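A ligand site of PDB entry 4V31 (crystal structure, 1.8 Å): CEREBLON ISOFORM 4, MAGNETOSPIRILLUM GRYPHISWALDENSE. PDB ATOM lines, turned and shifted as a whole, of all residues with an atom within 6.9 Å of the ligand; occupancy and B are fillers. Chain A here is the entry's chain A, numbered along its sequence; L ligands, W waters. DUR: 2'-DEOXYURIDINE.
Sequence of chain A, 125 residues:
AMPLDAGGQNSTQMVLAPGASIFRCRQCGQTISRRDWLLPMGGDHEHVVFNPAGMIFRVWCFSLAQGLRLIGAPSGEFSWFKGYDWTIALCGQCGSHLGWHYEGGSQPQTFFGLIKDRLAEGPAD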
ATOM      1  N   VAL A  49      34.343  31.393  19.022  1.00  0.00           N
ATOM      2  CA  VAL A  49      33.924  30.476  20.069  1.00  0.00           C
ATOM      3  C   VAL A  49      34.844  29.258  20.168  1.00  0.00           C
ATOM      4  O   VAL A  49      35.520  29.006  19.250  1.00  0.00           O
ATOM      5  CB  VAL A  49      32.484  30.026  19.779  1.00  0.00           C
ATOM      6  CG1 VAL A  49      31.566  31.224  19.729  1.00  0.00           C
ATOM      7  CG2 VAL A  49      32.365  29.261  18.453  1.00  0.00           C
ATOM      8  N   PHE A  50      34.755  28.477  21.235  1.00  0.00           N
ATOM      9  CA  PHE A  50      35.486  27.213  21.395  1.00  0.00           C
ATOM     10  C   PHE A  50      34.527  26.148  21.788  1.00  0.00           C
ATOM     11  O   PHE A  50      33.557  26.384  22.561  1.00  0.00           O
ATOM     12  CB  PHE A  50      36.524  27.257  22.532  1.00  0.00           C
ATOM     13  CG  PHE A  50      37.448  28.366  22.462  1.00  0.00           C
ATOM     14  CD1 PHE A  50      37.120  29.562  23.060  1.00  0.00           C
ATOM     15  CD2 PHE A  50      38.750  28.182  21.927  1.00  0.00           C
ATOM     16  CE1 PHE A  50      38.043  30.610  23.027  1.00  0.00           C
ATOM     17  CE2 PHE A  50      39.663  29.239  21.903  1.00  0.00           C
ATOM     18  CZ  PHE A  50      39.315  30.446  22.465  1.00  0.00           C
ATOM     19  N   ASN A  51      34.715  24.950  21.216  1.00  0.00           N
ATOM     20  CA  ASN A  51      33.987  23.808  21.669  1.00  0.00           C
ATOM     21  C   ASN A  51      34.644  23.178  22.944  1.00  0.00           C
ATOM     22  O   ASN A  51      35.725  23.635  23.404  1.00  0.00           O
ATOM     23  CB  ASN A  51      33.745  22.823  20.473  1.00  0.00           C
ATOM     24  CG  ASN A  51      35.008  22.218  19.969  1.00  0.00           C
ATOM     25  OD1 ASN A  51      36.052  22.280  20.637  1.00  0.00           O
ATOM     26  ND2 ASN A  51      34.927  21.555  18.800  1.00  0.00           N
ATOM     27  N   PRO A  52      33.988  22.132  23.542  1.00  0.00           N
ATOM     28  CA  PRO A  52      34.520  21.443  24.676  1.00  0.00           C
ATOM     29  C   PRO A  52      35.876  20.760  24.392  1.00  0.00           C
ATOM     30  O   PRO A  52      36.639  20.592  25.329  1.00  0.00           O
ATOM     31  CB  PRO A  52      33.413  20.459  25.040  1.00  0.00           C
ATOM     32  CG  PRO A  52      32.145  21.092  24.529  1.00  0.00           C
ATOM     33  CD  PRO A  52      32.606  21.674  23.227  1.00  0.00           C
ATOM     34  N   ALA A  53      36.199  20.482  23.136  1.00  0.00           N
ATOM     35  CA  ALA A  53      37.547  19.930  22.791  1.00  0.00           C
ATOM     36  C   ALA A  53      38.609  21.022  22.577  1.00  0.00           C
ATOM     37  O   ALA A  53      39.725  20.711  22.133  1.00  0.00           O
ATOM     38  CB  ALA A  53      37.492  19.057  21.565  1.00  0.00           C
ATOM     39  N   PHE A  57      36.687  28.499  16.688  1.00  0.00           N
ATOM     40  CA  PHE A  57      36.016  28.695  15.405  1.00  0.00           C
ATOM     41  C   PHE A  57      35.586  30.129  15.208  1.00  0.00           C
ATOM     42  O   PHE A  57      35.102  30.767  16.140  1.00  0.00           O
ATOM     43  CB  PHE A  57      34.708  27.909  15.325  1.00  0.00           C
ATOM     44  CG  PHE A  57      34.886  26.421  15.413  1.00  0.00           C
ATOM     45  CD1 PHE A  57      35.417  25.732  14.381  1.00  0.00           C
ATOM     46  CD2 PHE A  57      34.525  25.744  16.545  1.00  0.00           C
ATOM     47  CE1 PHE A  57      35.564  24.349  14.458  1.00  0.00           C
ATOM     48  CE2 PHE A  57      34.682  24.390  16.678  1.00  0.00           C
ATOM     49  CZ  PHE A  57      35.161  23.675  15.587  1.00  0.00           C
ATOM     50  N   SER A  75      20.052  20.140  19.975  1.00  0.00           N
ATOM     51  CA  SER A  75      20.528  20.029  21.335  1.00  0.00           C
ATOM     52  C   SER A  75      20.873  21.422  21.875  1.00  0.00           C
ATOM     53  O   SER A  75      21.473  22.229  21.136  1.00  0.00           O
ATOM     54  CB  SER A  75      21.814  19.168  21.414  1.00  0.00           C
ATOM     55  OG  SER A  75      22.258  19.204  22.797  1.00  0.00           O
ATOM     56  N   GLY A  76      20.524  21.706  23.112  1.00  0.00           N
ATOM     57  CA  GLY A  76      20.869  22.956  23.773  1.00  0.00           C
ATOM     58  C   GLY A  76      22.243  22.891  24.466  1.00  0.00           C
ATOM     59  O   GLY A  76      22.725  23.890  24.899  1.00  0.00           O
ATOM     60  N   GLU A  77      22.842  21.710  24.583  1.00  0.00           N
ATOM     61  CA  GLU A  77      24.110  21.566  25.301  1.00  0.00           C
ATOM     62  C   GLU A  77      25.223  22.429  24.791  1.00  0.00           C
ATOM     63  O   GLU A  77      25.488  22.424  23.654  1.00  0.00           O
ATOM     64  CB  GLU A  77      24.588  20.124  25.324  1.00  0.00           C
ATOM     65  CG  GLU A  77      23.486  19.112  25.382  1.00  0.00           C
ATOM     66  CD  GLU A  77      23.819  17.872  26.148  1.00  0.00           C
ATOM     67  OE1 GLU A  77      24.383  16.950  25.555  1.00  0.00           O
ATOM     68  OE2 GLU A  77      23.469  17.805  27.331  1.00  0.00           O
ATOM     69  N   PHE A  78      25.859  23.168  25.665  1.00  0.00           N
ATOM     70  CA  PHE A  78      26.997  24.058  25.283  1.00  0.00           C
ATOM     71  C   PHE A  78      26.715  25.122  24.225  1.00  0.00           C
ATOM     72  O   PHE A  78      27.626  25.697  23.639  1.00  0.00           O
ATOM     73  CB  PHE A  78      28.172  23.243  24.781  1.00  0.00           C
ATOM     74  CG  PHE A  78      28.602  22.128  25.688  1.00  0.00           C
ATOM     75  CD1 PHE A  78      29.112  22.399  26.925  1.00  0.00           C
ATOM     76  CD2 PHE A  78      28.487  20.830  25.284  1.00  0.00           C
ATOM     77  CE1 PHE A  78      29.504  21.394  27.764  1.00  0.00           C
ATOM     78  CE2 PHE A  78      28.864  19.787  26.117  1.00  0.00           C
ATOM     79  CZ  PHE A  78      29.380  20.069  27.349  1.00  0.00           C
ATOM     80  N   SER A  79      25.440  25.388  23.942  1.00  0.00           N
ATOM     81  CA  SER A  79      25.110  26.341  22.888  1.00  0.00           C
ATOM     82  C   SER A  79      25.793  27.691  23.093  1.00  0.00           C
ATOM     83  O   SER A  79      25.729  28.255  24.178  1.00  0.00           O
ATOM     84  CB  SER A  79      23.619  26.605  22.768  1.00  0.00           C
ATOM     85  OG  SER A  79      23.395  27.517  21.707  1.00  0.00           O
ATOM     86  N   TRP A  80      26.402  28.185  21.994  1.00  0.00           N
ATOM     87  CA  TRP A  80      27.122  29.466  22.015  1.00  0.00           C
ATOM     88  C   TRP A  80      26.196  30.643  21.911  1.00  0.00           C
ATOM     89  O   TRP A  80      26.615  31.746  22.043  1.00  0.00           O
ATOM     90  CB  TRP A  80      28.178  29.545  20.916  1.00  0.00           C
ATOM     91  CG  TRP A  80      29.253  28.580  20.997  1.00  0.00           C
ATOM     92  CD1 TRP A  80      30.094  28.372  22.049  1.00  0.00           C
ATOM     93  CD2 TRP A  80      29.685  27.714  19.974  1.00  0.00           C
ATOM     94  NE1 TRP A  80      30.983  27.364  21.760  1.00  0.00           N
ATOM     95  CE2 TRP A  80      30.813  26.999  20.463  1.00  0.00           C
ATOM     96  CE3 TRP A  80      29.262  27.479  18.669  1.00  0.00           C
ATOM     97  CZ2 TRP A  80      31.421  25.999  19.729  1.00  0.00           C
ATOM     98  CZ3 TRP A  80      29.902  26.533  17.942  1.00  0.00           C
ATOM     99  CH2 TRP A  80      30.984  25.807  18.465  1.00  0.00           C
ATOM    100  N   PHE A  81      24.909  30.404  21.676  1.00  0.00           N
ATOM    101  CA  PHE A  81      23.926  31.436  21.373  1.00  0.00           C
ATOM    102  C   PHE A  81      22.705  31.205  22.286  1.00  0.00           C
ATOM    103  O   PHE A  81      22.042  30.189  22.214  1.00  0.00           O
ATOM    104  CB  PHE A  81      23.506  31.401  19.888  1.00  0.00           C
ATOM    105  CG  PHE A  81      24.619  31.690  18.920  1.00  0.00           C
ATOM    106  CD1 PHE A  81      24.926  33.016  18.560  1.00  0.00           C
ATOM    107  CD2 PHE A  81      25.332  30.650  18.334  1.00  0.00           C
ATOM    108  CE1 PHE A  81      25.932  33.292  17.649  1.00  0.00           C
ATOM    109  CE2 PHE A  81      26.399  30.941  17.473  1.00  0.00           C
ATOM    110  CZ  PHE A  81      26.643  32.270  17.101  1.00  0.00           C
ATOM    111  N   TYR A  84      19.103  29.149  21.923  1.00  0.00           N
ATOM    112  CA  TYR A  84      19.062  28.332  20.687  1.00  0.00           C
ATOM    113  C   TYR A  84      19.616  26.960  20.938  1.00  0.00           C
ATOM    114  O   TYR A  84      20.599  26.803  21.715  1.00  0.00           O
ATOM    115  CB  TYR A  84      19.852  28.948  19.460  1.00  0.00           C
ATOM    116  CG  TYR A  84      19.316  30.343  19.034  1.00  0.00           C
ATOM    117  CD1 TYR A  84      19.777  31.512  19.668  1.00  0.00           C
ATOM    118  CD2 TYR A  84      18.352  30.483  18.048  1.00  0.00           C
ATOM    119  CE1 TYR A  84      19.280  32.768  19.302  1.00  0.00           C
ATOM    120  CE2 TYR A  84      17.867  31.719  17.691  1.00  0.00           C
ATOM    121  CZ  TYR A  84      18.396  32.870  18.289  1.00  0.00           C
ATOM    122  OH  TYR A  84      17.893  34.123  17.987  1.00  0.00           O
ATOM    123  N   ASP A  85      19.078  25.999  20.197  1.00  0.00           N
ATOM    124  CA  ASP A  85      19.554  24.675  20.156  1.00  0.00           C
ATOM    125  C   ASP A  85      20.152  24.442  18.804  1.00  0.00           C
ATOM    126  O   ASP A  85      19.688  24.979  17.815  1.00  0.00           O
ATOM    127  CB  ASP A  85      18.381  23.712  20.414  1.00  0.00           C
ATOM    128  CG  ASP A  85      17.521  24.167  21.629  1.00  0.00           C
ATOM    129  OD1 ASP A  85      18.121  24.414  22.724  1.00  0.00           O
ATOM    130  OD2 ASP A  85      16.291  24.435  21.440  1.00  0.00           O
ATOM    131  N   TRP A  86      21.190  23.611  18.757  1.00  0.00           N
ATOM    132  CA  TRP A  86      21.937  23.380  17.527  1.00  0.00           C
ATOM    133  C   TRP A  86      21.795  21.991  16.985  1.00  0.00           C
ATOM    134  O   TRP A  86      21.609  21.027  17.759  1.00  0.00           O
ATOM    135  CB  TRP A  86      23.427  23.727  17.703  1.00  0.00           C
ATOM    136  CG  TRP A  86      24.107  23.004  18.858  1.00  0.00           C
ATOM    137  CD1 TRP A  86      24.278  23.472  20.099  1.00  0.00           C
ATOM    138  CD2 TRP A  86      24.624  21.652  18.879  1.00  0.00           C
ATOM    139  NE1 TRP A  86      24.796  22.499  20.927  1.00  0.00           N
ATOM    140  CE2 TRP A  86      25.062  21.387  20.177  1.00  0.00           C
ATOM    141  CE3 TRP A  86      24.742  20.648  17.909  1.00  0.00           C
ATOM    142  CZ2 TRP A  86      25.608  20.188  20.535  1.00  0.00           C
ATOM    143  CZ3 TRP A  86      25.285  19.464  18.259  1.00  0.00           C
ATOM    144  CH2 TRP A  86      25.737  19.249  19.589  1.00  0.00           C
ATOM    145  N   THR A  87      21.940  21.913  15.660  1.00  0.00           N
ATOM    146  CA  THR A  87      22.028  20.683  14.841  1.00  0.00           C
ATOM    147  C   THR A  87      23.239  20.814  13.982  1.00  0.00           C
ATOM    148  O   THR A  87      23.456  21.823  13.345  1.00  0.00           O
ATOM    149  CB  THR A  87      20.759  20.571  13.954  1.00  0.00           C
ATOM    150  OG1 THR A  87      19.619  20.452  14.864  1.00  0.00           O
ATOM    151  CG2 THR A  87      20.802  19.392  13.234  1.00  0.00           C
ATOM    152  N   ILE A  88      24.054  19.786  13.926  1.00  0.00           N
ATOM    153  CA  ILE A  88      25.245  19.783  13.051  1.00  0.00           C
ATOM    154  C   ILE A  88      24.832  19.939  11.594  1.00  0.00           C
ATOM    155  O   ILE A  88      23.847  19.278  11.116  1.00  0.00           O
ATOM    156  CB  ILE A  88      26.023  18.479  13.271  1.00  0.00           C
ATOM    157  CG1 ILE A  88      26.703  18.587  14.630  1.00  0.00           C
ATOM    158  CG2 ILE A  88      26.982  18.209  12.106  1.00  0.00           C
ATOM    159  CD1 ILE A  88      27.418  17.334  15.066  1.00  0.00           C
ATOM    160  N   HIS A  97      32.161  19.189   7.626  1.00  0.00           N
ATOM    161  CA  HIS A  97      31.362  19.849   8.661  1.00  0.00           C
ATOM    162  C   HIS A  97      31.518  21.329   8.504  1.00  0.00           C
ATOM    163  O   HIS A  97      32.569  21.882   8.840  1.00  0.00           O
ATOM    164  CB  HIS A  97      31.806  19.389  10.012  1.00  0.00           C
ATOM    165  CG  HIS A  97      31.121  20.055  11.135  1.00  0.00           C
ATOM    166  ND1 HIS A  97      31.729  20.215  12.373  1.00  0.00           N
ATOM    167  CD2 HIS A  97      29.918  20.672  11.220  1.00  0.00           C
ATOM    168  CE1 HIS A  97      30.917  20.917  13.161  1.00  0.00           C
ATOM    169  NE2 HIS A  97      29.812  21.183  12.485  1.00  0.00           N
ATOM    170  N   GLY A  99      29.245  23.791   9.863  1.00  0.00           N
ATOM    171  CA  GLY A  99      28.748  24.544  10.960  1.00  0.00           C
ATOM    172  C   GLY A  99      27.553  23.902  11.598  1.00  0.00           C
ATOM    173  O   GLY A  99      27.507  22.709  11.797  1.00  0.00           O
ATOM    174  N   TRP A 100      26.588  24.767  11.960  1.00  0.00           N
ATOM    175  CA  TRP A 100      25.410  24.364  12.713  1.00  0.00           C
ATOM    176  C   TRP A 100      24.187  25.144  12.276  1.00  0.00           C
ATOM    177  O   TRP A 100      24.260  26.327  11.896  1.00  0.00           O
ATOM    178  CB  TRP A 100      25.604  24.544  14.238  1.00  0.00           C
ATOM    179  CG  TRP A 100      26.848  23.889  14.766  1.00  0.00           C
ATOM    180  CD1 TRP A 100      26.950  22.619  15.327  1.00  0.00           C
ATOM    181  CD2 TRP A 100      28.182  24.383  14.687  1.00  0.00           C
ATOM    182  NE1 TRP A 100      28.269  22.340  15.634  1.00  0.00           N
ATOM    183  CE2 TRP A 100      29.051  23.399  15.230  1.00  0.00           C
ATOM    184  CE3 TRP A 100      28.758  25.598  14.257  1.00  0.00           C
ATOM    185  CZ2 TRP A 100      30.445  23.612  15.340  1.00  0.00           C
ATOM    186  CZ3 TRP A 100      30.133  25.743  14.328  1.00  0.00           C
ATOM    187  CH2 TRP A 100      30.933  24.797  14.857  1.00  0.00           C
ATOM    188  N   TYR A 102      20.774  26.578  13.917  1.00  0.00           N
ATOM    189  CA  TYR A 102      20.255  26.944  15.218  1.00  0.00           C
ATOM    190  C   TYR A 102      18.752  27.254  15.132  1.00  0.00           C
ATOM    191  O   TYR A 102      18.312  27.832  14.164  1.00  0.00           O
ATOM    192  CB  TYR A 102      20.930  28.204  15.771  1.00  0.00           C
ATOM    193  CG  TYR A 102      22.339  27.960  16.276  1.00  0.00           C
ATOM    194  CD1 TYR A 102      22.602  27.470  17.540  1.00  0.00           C
ATOM    195  CD2 TYR A 102      23.408  28.160  15.387  1.00  0.00           C
ATOM    196  CE1 TYR A 102      23.949  27.207  17.950  1.00  0.00           C
ATOM    197  CE2 TYR A 102      24.723  27.903  15.754  1.00  0.00           C
ATOM    198  CZ  TYR A 102      24.992  27.401  17.016  1.00  0.00           C
ATOM    199  OH  TYR A 102      26.335  27.181  17.328  1.00  0.00           O
HETATM  200  N1  DUR L   1      29.100  22.891  19.972  1.00  0.00           N
HETATM  201  C2  DUR L   1      29.123  23.869  20.952  1.00  0.00           C
HETATM  202  N3  DUR L   1      28.305  24.916  20.914  1.00  0.00           N
HETATM  203  C4  DUR L   1      27.406  25.083  19.894  1.00  0.00           C
HETATM  204  C5  DUR L   1      27.348  24.133  18.876  1.00  0.00           C
HETATM  205  C6  DUR L   1      28.235  23.041  18.914  1.00  0.00           C
HETATM  206  O2  DUR L   1      29.947  23.757  21.873  1.00  0.00           O
HETATM  207  O4  DUR L   1      26.654  26.100  19.903  1.00  0.00           O
HETATM  208  C1' DUR L   1      30.009  21.785  20.081  1.00  0.00           C
HETATM  209  C2' DUR L   1      29.335  20.634  20.806  1.00  0.00           C
HETATM  210  C3' DUR L   1      29.826  19.392  20.142  1.00  0.00           C
HETATM  211  C4' DUR L   1      30.218  19.829  18.779  1.00  0.00           C
HETATM  212  O3' DUR L   1      30.921  18.901  20.977  1.00  0.00           O
HETATM  213  O4' DUR L   1      30.347  21.294  18.808  1.00  0.00           O
HETATM  214  C5' DUR L   1      29.181  19.384  17.728  1.00  0.00           C
HETATM  215  O5' DUR L   1      29.579  20.071  16.546  1.00  0.00           O
HETATM  216  O   HOH W   1      32.768  19.853  15.381  1.00  0.00           O
HETATM  217  O   HOH W   2      32.602  21.645  17.245  1.00  0.00           O
HETATM  218  O   HOH W   3      33.919  19.304  21.068  1.00  0.00           O
HETATM  219  O   HOH W   4      30.105  18.002  23.228  1.00  0.00           O
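The backbone NH (N) of Ala 53 is in hydrogen-bond range of the side-chain amide oxygen (OD1) of Asn 51 (3.1 Å).
The backbone carbonyl oxygen (O) of Tyr 84 lies within hydrogen-bond range of the side-chain hydroxyl (OG) of Ser 79, 2.9 Å away.
O of Glu 77 lies within hydrogen-bond range of NE1 of Trp 86 (2.8 Å).
A ring nitrogen (NE2) of His 97 sits at hydrogen-bond distance from the backbone carbonyl oxygen of Gly 99 (2.8 Å).
NE1 of Trp 80 is in hydrogen-bond range of O of Phe 50, 2.9 Å away.
OG of Ser 79 lies within hydrogen-bond range of O of Phe 81 (3.0 Å).
The backbone carbonyl oxygen (O) of Ser 75 lies within hydrogen-bond range of the backbone NH (N) of Trp 86 (2.8 Å).
The backbone carbonyl oxygen of Phe 78 sits at hydrogen-bond distance from a nitrogen (N3) of the ligand (2.9 Å).
The backbone NH (N) of Trp 80 lies within hydrogen-bond range of an oxygen (O4) of the ligand, at 3.0 Å.
The indole nitrogen of Trp 100 lies within hydrogen-bond range of an oxygen (O5') of the ligand (2.8 Å).
The side-chain hydroxyl of Tyr 102 sits at hydrogen-bond distance from an oxygen (O4) of the ligand (2.8 Å).
Asn 51 touches the ligand (CB to C1', 3.9 Å).
Pro 52 touches the ligand.
Ser 79 touches the ligand.
CD1 of Trp 86 touches C5 of the ligand, 3.4 Å away.
CG1 of Ile 88 touches O5' of the ligand, at 3.8 Å.
His 97 touches the ligand.
Within 4 Å of the ligand: Asn 51, Pro 52, Phe 78, Ser 79, Trp 80, Trp 86, Ile 88, His 97, Trp 100 and Tyr 102.
Along chain A the residues within 4 Å of the ligand span positions 51 to 102.
The nearest printed residue that does not touch the ligand is Phe 50 (4.5 Å).
Water W2 bridges an oxygen (O4') of the ligand (2.8 Å) and the side-chain amide nitrogen (ND2) of Asn 51 (2.8 Å).
Water W3 lies within hydrogen-bond range of O3' of the ligand (3.0 Å), N of Ala 53 (3.3 Å) and ND2 of Asn 51 (3.4 Å).
Water W1 lies within hydrogen-bond range of a ring nitrogen (ND1) of His 97 and an oxygen (O5') of the ligand.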
